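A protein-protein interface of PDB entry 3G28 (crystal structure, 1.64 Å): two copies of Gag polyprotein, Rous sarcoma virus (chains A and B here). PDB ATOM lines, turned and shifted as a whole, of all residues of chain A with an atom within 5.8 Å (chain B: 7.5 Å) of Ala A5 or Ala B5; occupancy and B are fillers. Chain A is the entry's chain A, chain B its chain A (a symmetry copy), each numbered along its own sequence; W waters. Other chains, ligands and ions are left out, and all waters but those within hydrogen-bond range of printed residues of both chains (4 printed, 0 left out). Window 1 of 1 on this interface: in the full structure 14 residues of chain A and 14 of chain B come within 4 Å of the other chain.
O of Ala B5 lies within hydrogen-bond range of NZ of Lys A47, 2.8 Å away.
The backbone NH of Trp B4 is in hydrogen-bond range of the side-chain amide oxygen of Gln A46, at 3.4 Å.
The backbone NH (N) of Trp A4 sits at hydrogen-bond distance from the side-chain amide oxygen (OE1) of Gln B46 (3.4 Å).
The side-chain amide oxygen of Gln A46 is in hydrogen-bond range of the backbone NH of Ala B5.
The backbone carbonyl oxygen of Ala A5 sits at hydrogen-bond distance from the side-chain amino group of Lys B47, 2.8 Å away.
The side-chain carboxylate (OD2) of Asp A42 lies within hydrogen-bond range of the indole nitrogen (NE1) of Trp B4 (3.2 Å).
NE1 of Trp A4 is in hydrogen-bond range of OD2 of Asp B42, at 3.2 Å.
N of Ala A5 lies within hydrogen-bond range of OE1 of Gln B46, at 2.8 Å.
The backbone carbonyl oxygen of Ala B5 lies within hydrogen-bond range of the side-chain amino group of Lys B47, at 2.9 Å.
The backbone carbonyl oxygen (O) of Ala A5 sits at hydrogen-bond distance from the side-chain amino group (NZ) of Lys A47 (2.9 Å).
Among the printed residues, merely in contact across the chains: Gln A46 with Pro B3, Pro A3 with Gln B46, Lys A47 with Asp B6, Asp A6 with Lys B47, Gln A46 with Asp B6, Asp A6 with Gln B46, Trp A4 with Trp B4, Ala A5 with Ala B5 and Lys A47 with Lys B47.
Of the printed residues of chain B, Ala A5 touches Ala B5 (3.8 Å), Gln B46 (2.8 Å) and Lys B47 (2.8 Å).
Of the printed residues of chain B, Asp A6 touches Gln B46 (3.5 Å) and Lys B47 (3.3 Å).
Of the printed residues of chain A, Pro B3 touches Gln A46 (3.2 Å).
Of the printed residues of chain A, Gln B46 touches Pro A3 (3.2 Å), Trp A4 (3.4 Å), Ala A5 (2.8 Å) and Asp A6 (3.5 Å).
Of the printed residues of chain B, Asp A42 touches Trp B4 (3.2 Å).
Printed residues of chain B within 4 Å of Trp A4: Trp B4 (3.6 Å), Asp B42 (3.2 Å) and Gln B46 (3.4 Å).
Val B26 touches none of the printed residues of chain A.
The nearest printed residue of chain A that does not touch Pro B3 is Lys A47 (6.9 Å).
Hydrophobic or aromatic side chains of chain A that line the printed part of chain B: Pro A3, Trp A4 and Ala A5.
Along chain A the printed residues that touch a printed residue of chain B span positions 3 to 47.
Of the 16 printed residues of chain B, 7 touch a printed residue of chain A.
Printed residues of chain B that touch a printed residue of chain A: Pro B3, Trp B4, Ala B5, Asp B6, Asp B42, Gln B46 and Lys B47.
Hydrophobic or aromatic side chains of chain B that line the printed part of chain A: Pro B3, Trp B4 and Ala B5.
Among the printed residues, no Asp or Glu carboxylate lies within 4 Å of a Lys or Arg side-chain nitrogen of the other chain.
Pro A3 touches Gln B46, and with the chains exchanged Gln A46 touches Pro B3.
Trp A4 touches Asp B42, and with the chains exchanged Asp A42 touches Trp B4.
Asp A6 touches Gln B46, and with the chains exchanged Gln A46 touches Asp B6.
Asp A6 touches Lys B47, and with the chains exchanged Lys A47 touches Asp B6.
Of the 17 pairs that touch across the chains among the printed residues, 17 have their exchanged pair printed and touching as well.
Water W4 bridges OD2 of Asp B6 (2.5 Å) and O of Gln A46 (2.7 Å).
Water W2 bridges OD2 of Asp A6 (2.5 Å) and O of Gln B46 (2.7 Å).
Water W3 lies within hydrogen-bond range of the backbone carbonyl oxygen (O) of Gln A46 and the side-chain carboxylate (OD1) of Asp B6.
Water W1 bridges O of Gln B46 and OD1 of Asp A6.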
ATOM      1  N   GLY A   2      12.814  25.201   6.154  1.00  0.00           N
ATOM      2  CA  GLY A   2      14.057  25.815   6.623  1.00  0.00           C
ATOM      3  C   GLY A   2      14.995  24.755   7.172  1.00  0.00           C
ATOM      4  O   GLY A   2      14.525  23.748   7.702  1.00  0.00           O
ATOM      5  N   PRO A   3      16.328  24.972   7.065  1.00  0.00           N
ATOM      6  CA  PRO A   3      17.220  23.974   7.635  1.00  0.00           C
ATOM      7  C   PRO A   3      17.195  24.134   9.145  1.00  0.00           C
ATOM      8  O   PRO A   3      17.869  24.980   9.719  1.00  0.00           O
ATOM      9  CB  PRO A   3      18.579  24.283   6.995  1.00  0.00           C
ATOM     10  CG  PRO A   3      18.421  25.749   6.427  1.00  0.00           C
ATOM     11  CD  PRO A   3      17.043  26.218   6.770  1.00  0.00           C
ATOM     12  N   TRP A   4      16.356  23.321   9.767  1.00  0.00           N
ATOM     13  CA  TRP A   4      16.081  23.462  11.180  1.00  0.00           C
ATOM     14  C   TRP A   4      17.343  23.378  12.048  1.00  0.00           C
ATOM     15  O   TRP A   4      17.405  24.016  13.104  1.00  0.00           O
ATOM     16  CB  TRP A   4      15.030  22.436  11.615  1.00  0.00           C
ATOM     17  CG  TRP A   4      15.489  20.992  11.524  1.00  0.00           C
ATOM     18  CD1 TRP A   4      15.243  20.104  10.491  1.00  0.00           C
ATOM     19  CD2 TRP A   4      16.248  20.268  12.503  1.00  0.00           C
ATOM     20  NE1 TRP A   4      15.819  18.892  10.772  1.00  0.00           N
ATOM     21  CE2 TRP A   4      16.428  18.951  12.001  1.00  0.00           C
ATOM     22  CE3 TRP A   4      16.798  20.603  13.758  1.00  0.00           C
ATOM     23  CZ2 TRP A   4      17.128  17.968  12.704  1.00  0.00           C
ATOM     24  CZ3 TRP A   4      17.498  19.625  14.467  1.00  0.00           C
ATOM     25  CH2 TRP A   4      17.659  18.314  13.933  1.00  0.00           C
ATOM     26  N   ALA A   5      18.353  22.605  11.635  1.00  0.00           N
ATOM     27  CA  ALA A   5      19.531  22.466  12.512  1.00  0.00           C
ATOM     28  C   ALA A   5      20.506  23.644  12.390  1.00  0.00           C
ATOM     29  O   ALA A   5      21.530  23.651  13.078  1.00  0.00           O
ATOM     30  CB  ALA A   5      20.269  21.140  12.227  1.00  0.00           C
ATOM     31  N   ASP A   6      20.219  24.608  11.505  1.00  0.00           N
ATOM     32  CA  ASP A   6      21.082  25.792  11.301  1.00  0.00           C
ATOM     33  C   ASP A   6      20.524  26.989  12.065  1.00  0.00           C
ATOM     34  O   ASP A   6      21.172  28.042  12.144  1.00  0.00           O
ATOM     35  CB  ASP A   6      21.104  26.263   9.841  1.00  0.00           C
ATOM     36  CG  ASP A   6      21.880  25.384   8.917  1.00  0.00           C
ATOM     37  OD1 ASP A   6      22.702  24.571   9.366  1.00  0.00           O
ATOM     38  OD2 ASP A   6      21.657  25.571   7.694  1.00  0.00           O
ATOM     39  N   ILE A   7      19.322  26.853  12.602  1.00  0.00           N
ATOM     40  CA  ILE A   7      18.634  28.029  13.108  1.00  0.00           C
ATOM     41  C   ILE A   7      19.173  28.405  14.492  1.00  0.00           C
ATOM     42  O   ILE A   7      19.215  27.566  15.413  1.00  0.00           O
ATOM     43  CB  ILE A   7      17.112  27.790  13.139  1.00  0.00           C
ATOM     44  CG1 ILE A   7      16.568  27.826  11.707  1.00  0.00           C
ATOM     45  CG2 ILE A   7      16.380  28.871  13.971  1.00  0.00           C
ATOM     46  CD1 ILE A   7      15.208  27.253  11.596  1.00  0.00           C
ATOM     47  N   ASP A  42      15.714  20.874  22.731  1.00  0.00           N
ATOM     48  CA  ASP A  42      17.184  20.900  22.658  1.00  0.00           C
ATOM     49  C   ASP A  42      17.716  22.087  21.871  1.00  0.00           C
ATOM     50  O   ASP A  42      18.746  22.663  22.233  1.00  0.00           O
ATOM     51  CB  ASP A  42      17.698  19.587  22.090  1.00  0.00           C
ATOM     52  CG  ASP A  42      17.535  18.433  23.065  1.00  0.00           C
ATOM     53  OD1 ASP A  42      17.128  18.674  24.231  1.00  0.00           O
ATOM     54  OD2 ASP A  42      17.794  17.273  22.662  1.00  0.00           O
ATOM     55  N   CYS A  43      17.032  22.457  20.776  1.00  0.00           N
ATOM     56  CA  CYS A  43      17.492  23.609  20.004  1.00  0.00           C
ATOM     57  C   CYS A  43      17.254  24.911  20.803  1.00  0.00           C
ATOM     58  O   CYS A  43      18.060  25.824  20.737  1.00  0.00           O
ATOM     59  CB  CYS A  43      16.834  23.654  18.621  1.00  0.00           C
ATOM     60  SG  CYS A  43      17.458  22.339  17.547  1.00  0.00           S
ATOM     61  N   GLN A  46      20.267  24.926  23.193  1.00  0.00           N
ATOM     62  CA  GLN A  46      21.597  25.030  22.603  1.00  0.00           C
ATOM     63  C   GLN A  46      21.787  26.208  21.656  1.00  0.00           C
ATOM     64  O   GLN A  46      22.914  26.649  21.472  1.00  0.00           O
ATOM     65  CB  GLN A  46      21.907  23.765  21.809  1.00  0.00           C
ATOM     66  CG  GLN A  46      22.018  22.544  22.667  1.00  0.00           C
ATOM     67  CD  GLN A  46      22.200  21.281  21.856  1.00  0.00           C
ATOM     68  OE1 GLN A  46      22.848  21.289  20.813  1.00  0.00           O
ATOM     69  NE2 GLN A  46      21.620  20.183  22.333  1.00  0.00           N
ATOM     70  N   LYS A  47      20.698  26.710  21.068  1.00  0.00           N
ATOM     71  CA  LYS A  47      20.803  27.608  19.918  1.00  0.00           C
ATOM     72  C   LYS A  47      20.235  29.005  20.169  1.00  0.00           C
ATOM     73  O   LYS A  47      20.276  29.876  19.294  1.00  0.00           O
ATOM     74  CB  LYS A  47      20.095  26.978  18.692  1.00  0.00           C
ATOM     75  CG  LYS A  47      20.473  25.507  18.419  1.00  0.00           C
ATOM     76  CD  LYS A  47      21.948  25.393  18.079  1.00  0.00           C
ATOM     77  CE  LYS A  47      22.291  25.983  16.693  1.00  0.00           C
ATOM     78  NZ  LYS A  47      21.972  25.007  15.632  1.00  0.00           N
ATOM     79  N   GLY B   2      27.888  16.150  24.231  1.00  0.00           N
ATOM     80  CA  GLY B   2      28.169  17.304  23.376  1.00  0.00           C
ATOM     81  C   GLY B   2      26.873  17.950  22.917  1.00  0.00           C
ATOM     82  O   GLY B   2      25.872  17.250  22.759  1.00  0.00           O
ATOM     83  N   PRO B   3      26.878  19.285  22.686  1.00  0.00           N
ATOM     84  CA  PRO B   3      25.646  19.888  22.202  1.00  0.00           C
ATOM     85  C   PRO B   3      25.487  19.515  20.738  1.00  0.00           C
ATOM     86  O   PRO B   3      26.066  20.123  19.847  1.00  0.00           O
ATOM     87  CB  PRO B   3      25.847  21.389  22.447  1.00  0.00           C
ATOM     88  CG  PRO B   3      27.404  21.546  22.661  1.00  0.00           C
ATOM     89  CD  PRO B   3      28.019  20.190  22.511  1.00  0.00           C
ATOM     90  N   TRP B   4      24.716  18.461  20.523  1.00  0.00           N
ATOM     91  CA  TRP B   4      24.602  17.868  19.209  1.00  0.00           C
ATOM     92  C   TRP B   4      24.125  18.862  18.143  1.00  0.00           C
ATOM     93  O   TRP B   4      24.506  18.739  16.974  1.00  0.00           O
ATOM     94  CB  TRP B   4      23.701  16.630  19.268  1.00  0.00           C
ATOM     95  CG  TRP B   4      22.253  16.926  19.609  1.00  0.00           C
ATOM     96  CD1 TRP B   4      21.657  16.836  20.856  1.00  0.00           C
ATOM     97  CD2 TRP B   4      21.221  17.333  18.699  1.00  0.00           C
ATOM     98  NE1 TRP B   4      20.333  17.181  20.763  1.00  0.00           N
ATOM     99  CE2 TRP B   4      20.027  17.474  19.457  1.00  0.00           C
ATOM    100  CE3 TRP B   4      21.187  17.596  17.314  1.00  0.00           C
ATOM    101  CZ2 TRP B   4      18.814  17.862  18.884  1.00  0.00           C
ATOM    102  CZ3 TRP B   4      19.976  17.982  16.733  1.00  0.00           C
ATOM    103  CH2 TRP B   4      18.799  18.115  17.525  1.00  0.00           C
ATOM    104  N   ALA B   5      23.295  19.844  18.510  1.00  0.00           N
ATOM    105  CA  ALA B   5      22.776  20.749  17.466  1.00  0.00           C
ATOM    106  C   ALA B   5      23.770  21.855  17.090  1.00  0.00           C
ATOM    107  O   ALA B   5      23.459  22.674  16.221  1.00  0.00           O
ATOM    108  CB  ALA B   5      21.434  21.374  17.903  1.00  0.00           C
ATOM    109  N   ASP B   6      24.933  21.907  17.753  1.00  0.00           N
ATOM    110  CA  ASP B   6      25.970  22.926  17.476  1.00  0.00           C
ATOM    111  C   ASP B   6      27.057  22.343  16.579  1.00  0.00           C
ATOM    112  O   ASP B   6      27.943  23.071  16.112  1.00  0.00           O
ATOM    113  CB  ASP B   6      26.726  23.357  18.739  1.00  0.00           C
ATOM    114  CG  ASP B   6      25.942  24.228  19.666  1.00  0.00           C
ATOM    115  OD1 ASP B   6      24.924  24.814  19.266  1.00  0.00           O
ATOM    116  OD2 ASP B   6      26.416  24.333  20.825  1.00  0.00           O
ATOM    117  N   ILE B   7      27.017  21.039  16.355  1.00  0.00           N
ATOM    118  CA  ILE B   7      28.160  20.390  15.734  1.00  0.00           C
ATOM    119  C   ILE B   7      28.140  20.617  14.219  1.00  0.00           C
ATOM    120  O   ILE B   7      27.132  20.334  13.543  1.00  0.00           O
ATOM    121  CB  ILE B   7      28.182  18.890  16.083  1.00  0.00           C
ATOM    122  CG1 ILE B   7      28.610  18.719  17.544  1.00  0.00           C
ATOM    123  CG2 ILE B   7      29.173  18.109  15.186  1.00  0.00           C
ATOM    124  CD1 ILE B   7      28.314  17.369  18.074  1.00  0.00           C
ATOM    125  N   MET B   8      29.252  21.126  13.703  1.00  0.00           N
ATOM    126  CA  MET B   8      29.367  21.370  12.257  1.00  0.00           C
ATOM    127  C   MET B   8      30.768  21.021  11.805  1.00  0.00           C
ATOM    128  O   MET B   8      31.734  21.182  12.553  1.00  0.00           O
ATOM    129  CB  MET B   8      28.999  22.809  11.897  1.00  0.00           C
ATOM    130  CG  MET B   8      29.800  23.867  12.624  1.00  0.00           C
ATOM    131  SD  MET B   8      29.332  25.493  11.987  1.00  0.00           S
ATOM    132  CE  MET B   8      27.550  25.476  12.115  1.00  0.00           C
ATOM    133  N   LEU B  22      29.410  14.081  15.696  1.00  0.00           N
ATOM    134  CA  LEU B  22      27.963  14.253  15.670  1.00  0.00           C
ATOM    135  C   LEU B  22      27.265  13.045  16.259  1.00  0.00           C
ATOM    136  O   LEU B  22      26.362  13.171  17.104  1.00  0.00           O
ATOM    137  CB  LEU B  22      27.492  14.511  14.227  1.00  0.00           C
ATOM    138  CG  LEU B  22      25.986  14.565  14.032  1.00  0.00           C
ATOM    139  CD1 LEU B  22      25.393  15.810  14.726  1.00  0.00           C
ATOM    140  CD2 LEU B  22      25.698  14.501  12.541  1.00  0.00           C
ATOM    141  N   ALA B  25      27.658  12.627  20.005  1.00  0.00           N
ATOM    142  CA  ALA B  25      26.786  13.579  20.677  1.00  0.00           C
ATOM    143  C   ALA B  25      25.321  13.154  20.658  1.00  0.00           C
ATOM    144  O   ALA B  25      24.601  13.267  21.671  1.00  0.00           O
ATOM    145  CB  ALA B  25      26.929  14.936  20.018  1.00  0.00           C
ATOM    146  N   VAL B  26      24.848  12.692  19.505  1.00  0.00           N
ATOM    147  CA  VAL B  26      23.466  12.268  19.390  1.00  0.00           C
ATOM    148  C   VAL B  26      23.199  11.045  20.267  1.00  0.00           C
ATOM    149  O   VAL B  26      22.185  10.973  20.948  1.00  0.00           O
ATOM    150  CB  VAL B  26      23.062  12.061  17.905  1.00  0.00           C
ATOM    151  CG1 VAL B  26      21.718  11.313  17.784  1.00  0.00           C
ATOM    152  CG2 VAL B  26      23.005  13.424  17.191  1.00  0.00           C
ATOM    153  N   VAL B  39      17.732  12.548  12.948  1.00  0.00           N
ATOM    154  CA  VAL B  39      18.511  13.702  13.354  1.00  0.00           C
ATOM    155  C   VAL B  39      19.919  13.648  12.756  1.00  0.00           C
ATOM    156  O   VAL B  39      20.408  14.651  12.239  1.00  0.00           O
ATOM    157  CB  VAL B  39      18.547  13.826  14.894  1.00  0.00           C
ATOM    158  CG1 VAL B  39      19.646  14.735  15.301  1.00  0.00           C
ATOM    159  CG2 VAL B  39      17.211  14.396  15.344  1.00  0.00           C
ATOM    160  N   ASP B  42      19.747  14.398   8.979  1.00  0.00           N
ATOM    161  CA  ASP B  42      19.538  15.834   8.734  1.00  0.00           C
ATOM    162  C   ASP B  42      20.755  16.677   9.077  1.00  0.00           C
ATOM    163  O   ASP B  42      21.058  17.648   8.378  1.00  0.00           O
ATOM    164  CB  ASP B  42      18.306  16.314   9.483  1.00  0.00           C
ATOM    165  CG  ASP B  42      17.018  15.784   8.875  1.00  0.00           C
ATOM    166  OD1 ASP B  42      17.074  15.136   7.798  1.00  0.00           O
ATOM    167  OD2 ASP B  42      15.941  15.996   9.484  1.00  0.00           O
ATOM    168  N   CYS B  43      21.458  16.329  10.167  1.00  0.00           N
ATOM    169  CA  CYS B  43      22.651  17.094  10.521  1.00  0.00           C
ATOM    170  C   CYS B  43      23.777  16.823   9.498  1.00  0.00           C
ATOM    171  O   CYS B  43      24.533  17.721   9.169  1.00  0.00           O
ATOM    172  CB  CYS B  43      23.097  16.803  11.959  1.00  0.00           C
ATOM    173  SG  CYS B  43      21.950  17.511  13.164  1.00  0.00           S
ATOM    174  N   PHE B  44      23.842  15.613   8.938  1.00  0.00           N
ATOM    175  CA  PHE B  44      24.791  15.386   7.834  1.00  0.00           C
ATOM    176  C   PHE B  44      24.434  16.326   6.669  1.00  0.00           C
ATOM    177  O   PHE B  44      25.316  16.941   6.073  1.00  0.00           O
ATOM    178  CB  PHE B  44      24.716  13.972   7.263  1.00  0.00           C
ATOM    179  CG  PHE B  44      25.390  12.878   8.091  1.00  0.00           C
ATOM    180  CD1 PHE B  44      26.111  13.139   9.265  1.00  0.00           C
ATOM    181  CD2 PHE B  44      25.293  11.555   7.639  1.00  0.00           C
ATOM    182  CE1 PHE B  44      26.723  12.067   9.962  1.00  0.00           C
ATOM    183  CE2 PHE B  44      25.906  10.491   8.323  1.00  0.00           C
ATOM    184  CZ  PHE B  44      26.616  10.760   9.470  1.00  0.00           C
ATOM    185  N   GLN B  46      22.777  19.143   6.598  1.00  0.00           N
ATOM    186  CA  GLN B  46      22.775  20.579   6.852  1.00  0.00           C
ATOM    187  C   GLN B  46      24.075  21.131   7.422  1.00  0.00           C
ATOM    188  O   GLN B  46      24.348  22.312   7.252  1.00  0.00           O
ATOM    189  CB  GLN B  46      21.671  20.924   7.847  1.00  0.00           C
ATOM    190  CG  GLN B  46      20.297  20.678   7.309  1.00  0.00           C
ATOM    191  CD  GLN B  46      19.220  20.904   8.347  1.00  0.00           C
ATOM    192  OE1 GLN B  46      19.337  21.782   9.196  1.00  0.00           O
ATOM    193  NE2 GLN B  46      18.161  20.101   8.284  1.00  0.00           N
ATOM    194  N   LYS B  47      24.868  20.284   8.085  1.00  0.00           N
ATOM    195  CA  LYS B  47      25.956  20.771   8.933  1.00  0.00           C
ATOM    196  C   LYS B  47      27.345  20.326   8.474  1.00  0.00           C
ATOM    197  O   LYS B  47      28.360  20.681   9.083  1.00  0.00           O
ATOM    198  CB  LYS B  47      25.728  20.314  10.397  1.00  0.00           C
ATOM    199  CG  LYS B  47      24.304  20.572  10.934  1.00  0.00           C
ATOM    200  CD  LYS B  47      24.015  22.062  10.974  1.00  0.00           C
ATOM    201  CE  LYS B  47      24.815  22.799  12.070  1.00  0.00           C
ATOM    202  NZ  LYS B  47      24.153  22.636  13.380  1.00  0.00           N
HETATM  203  O   HOH W   1      26.036  24.629   8.962  1.00  0.00           O
HETATM  204  O   HOH W   2      22.760  24.063   6.011  1.00  0.00           O
HETATM  205  O   HOH W   3      24.498  28.129  18.934  1.00  0.00           O
HETATM  206  O   HOH W   4      25.130  25.628  22.554  1.00  0.00           O
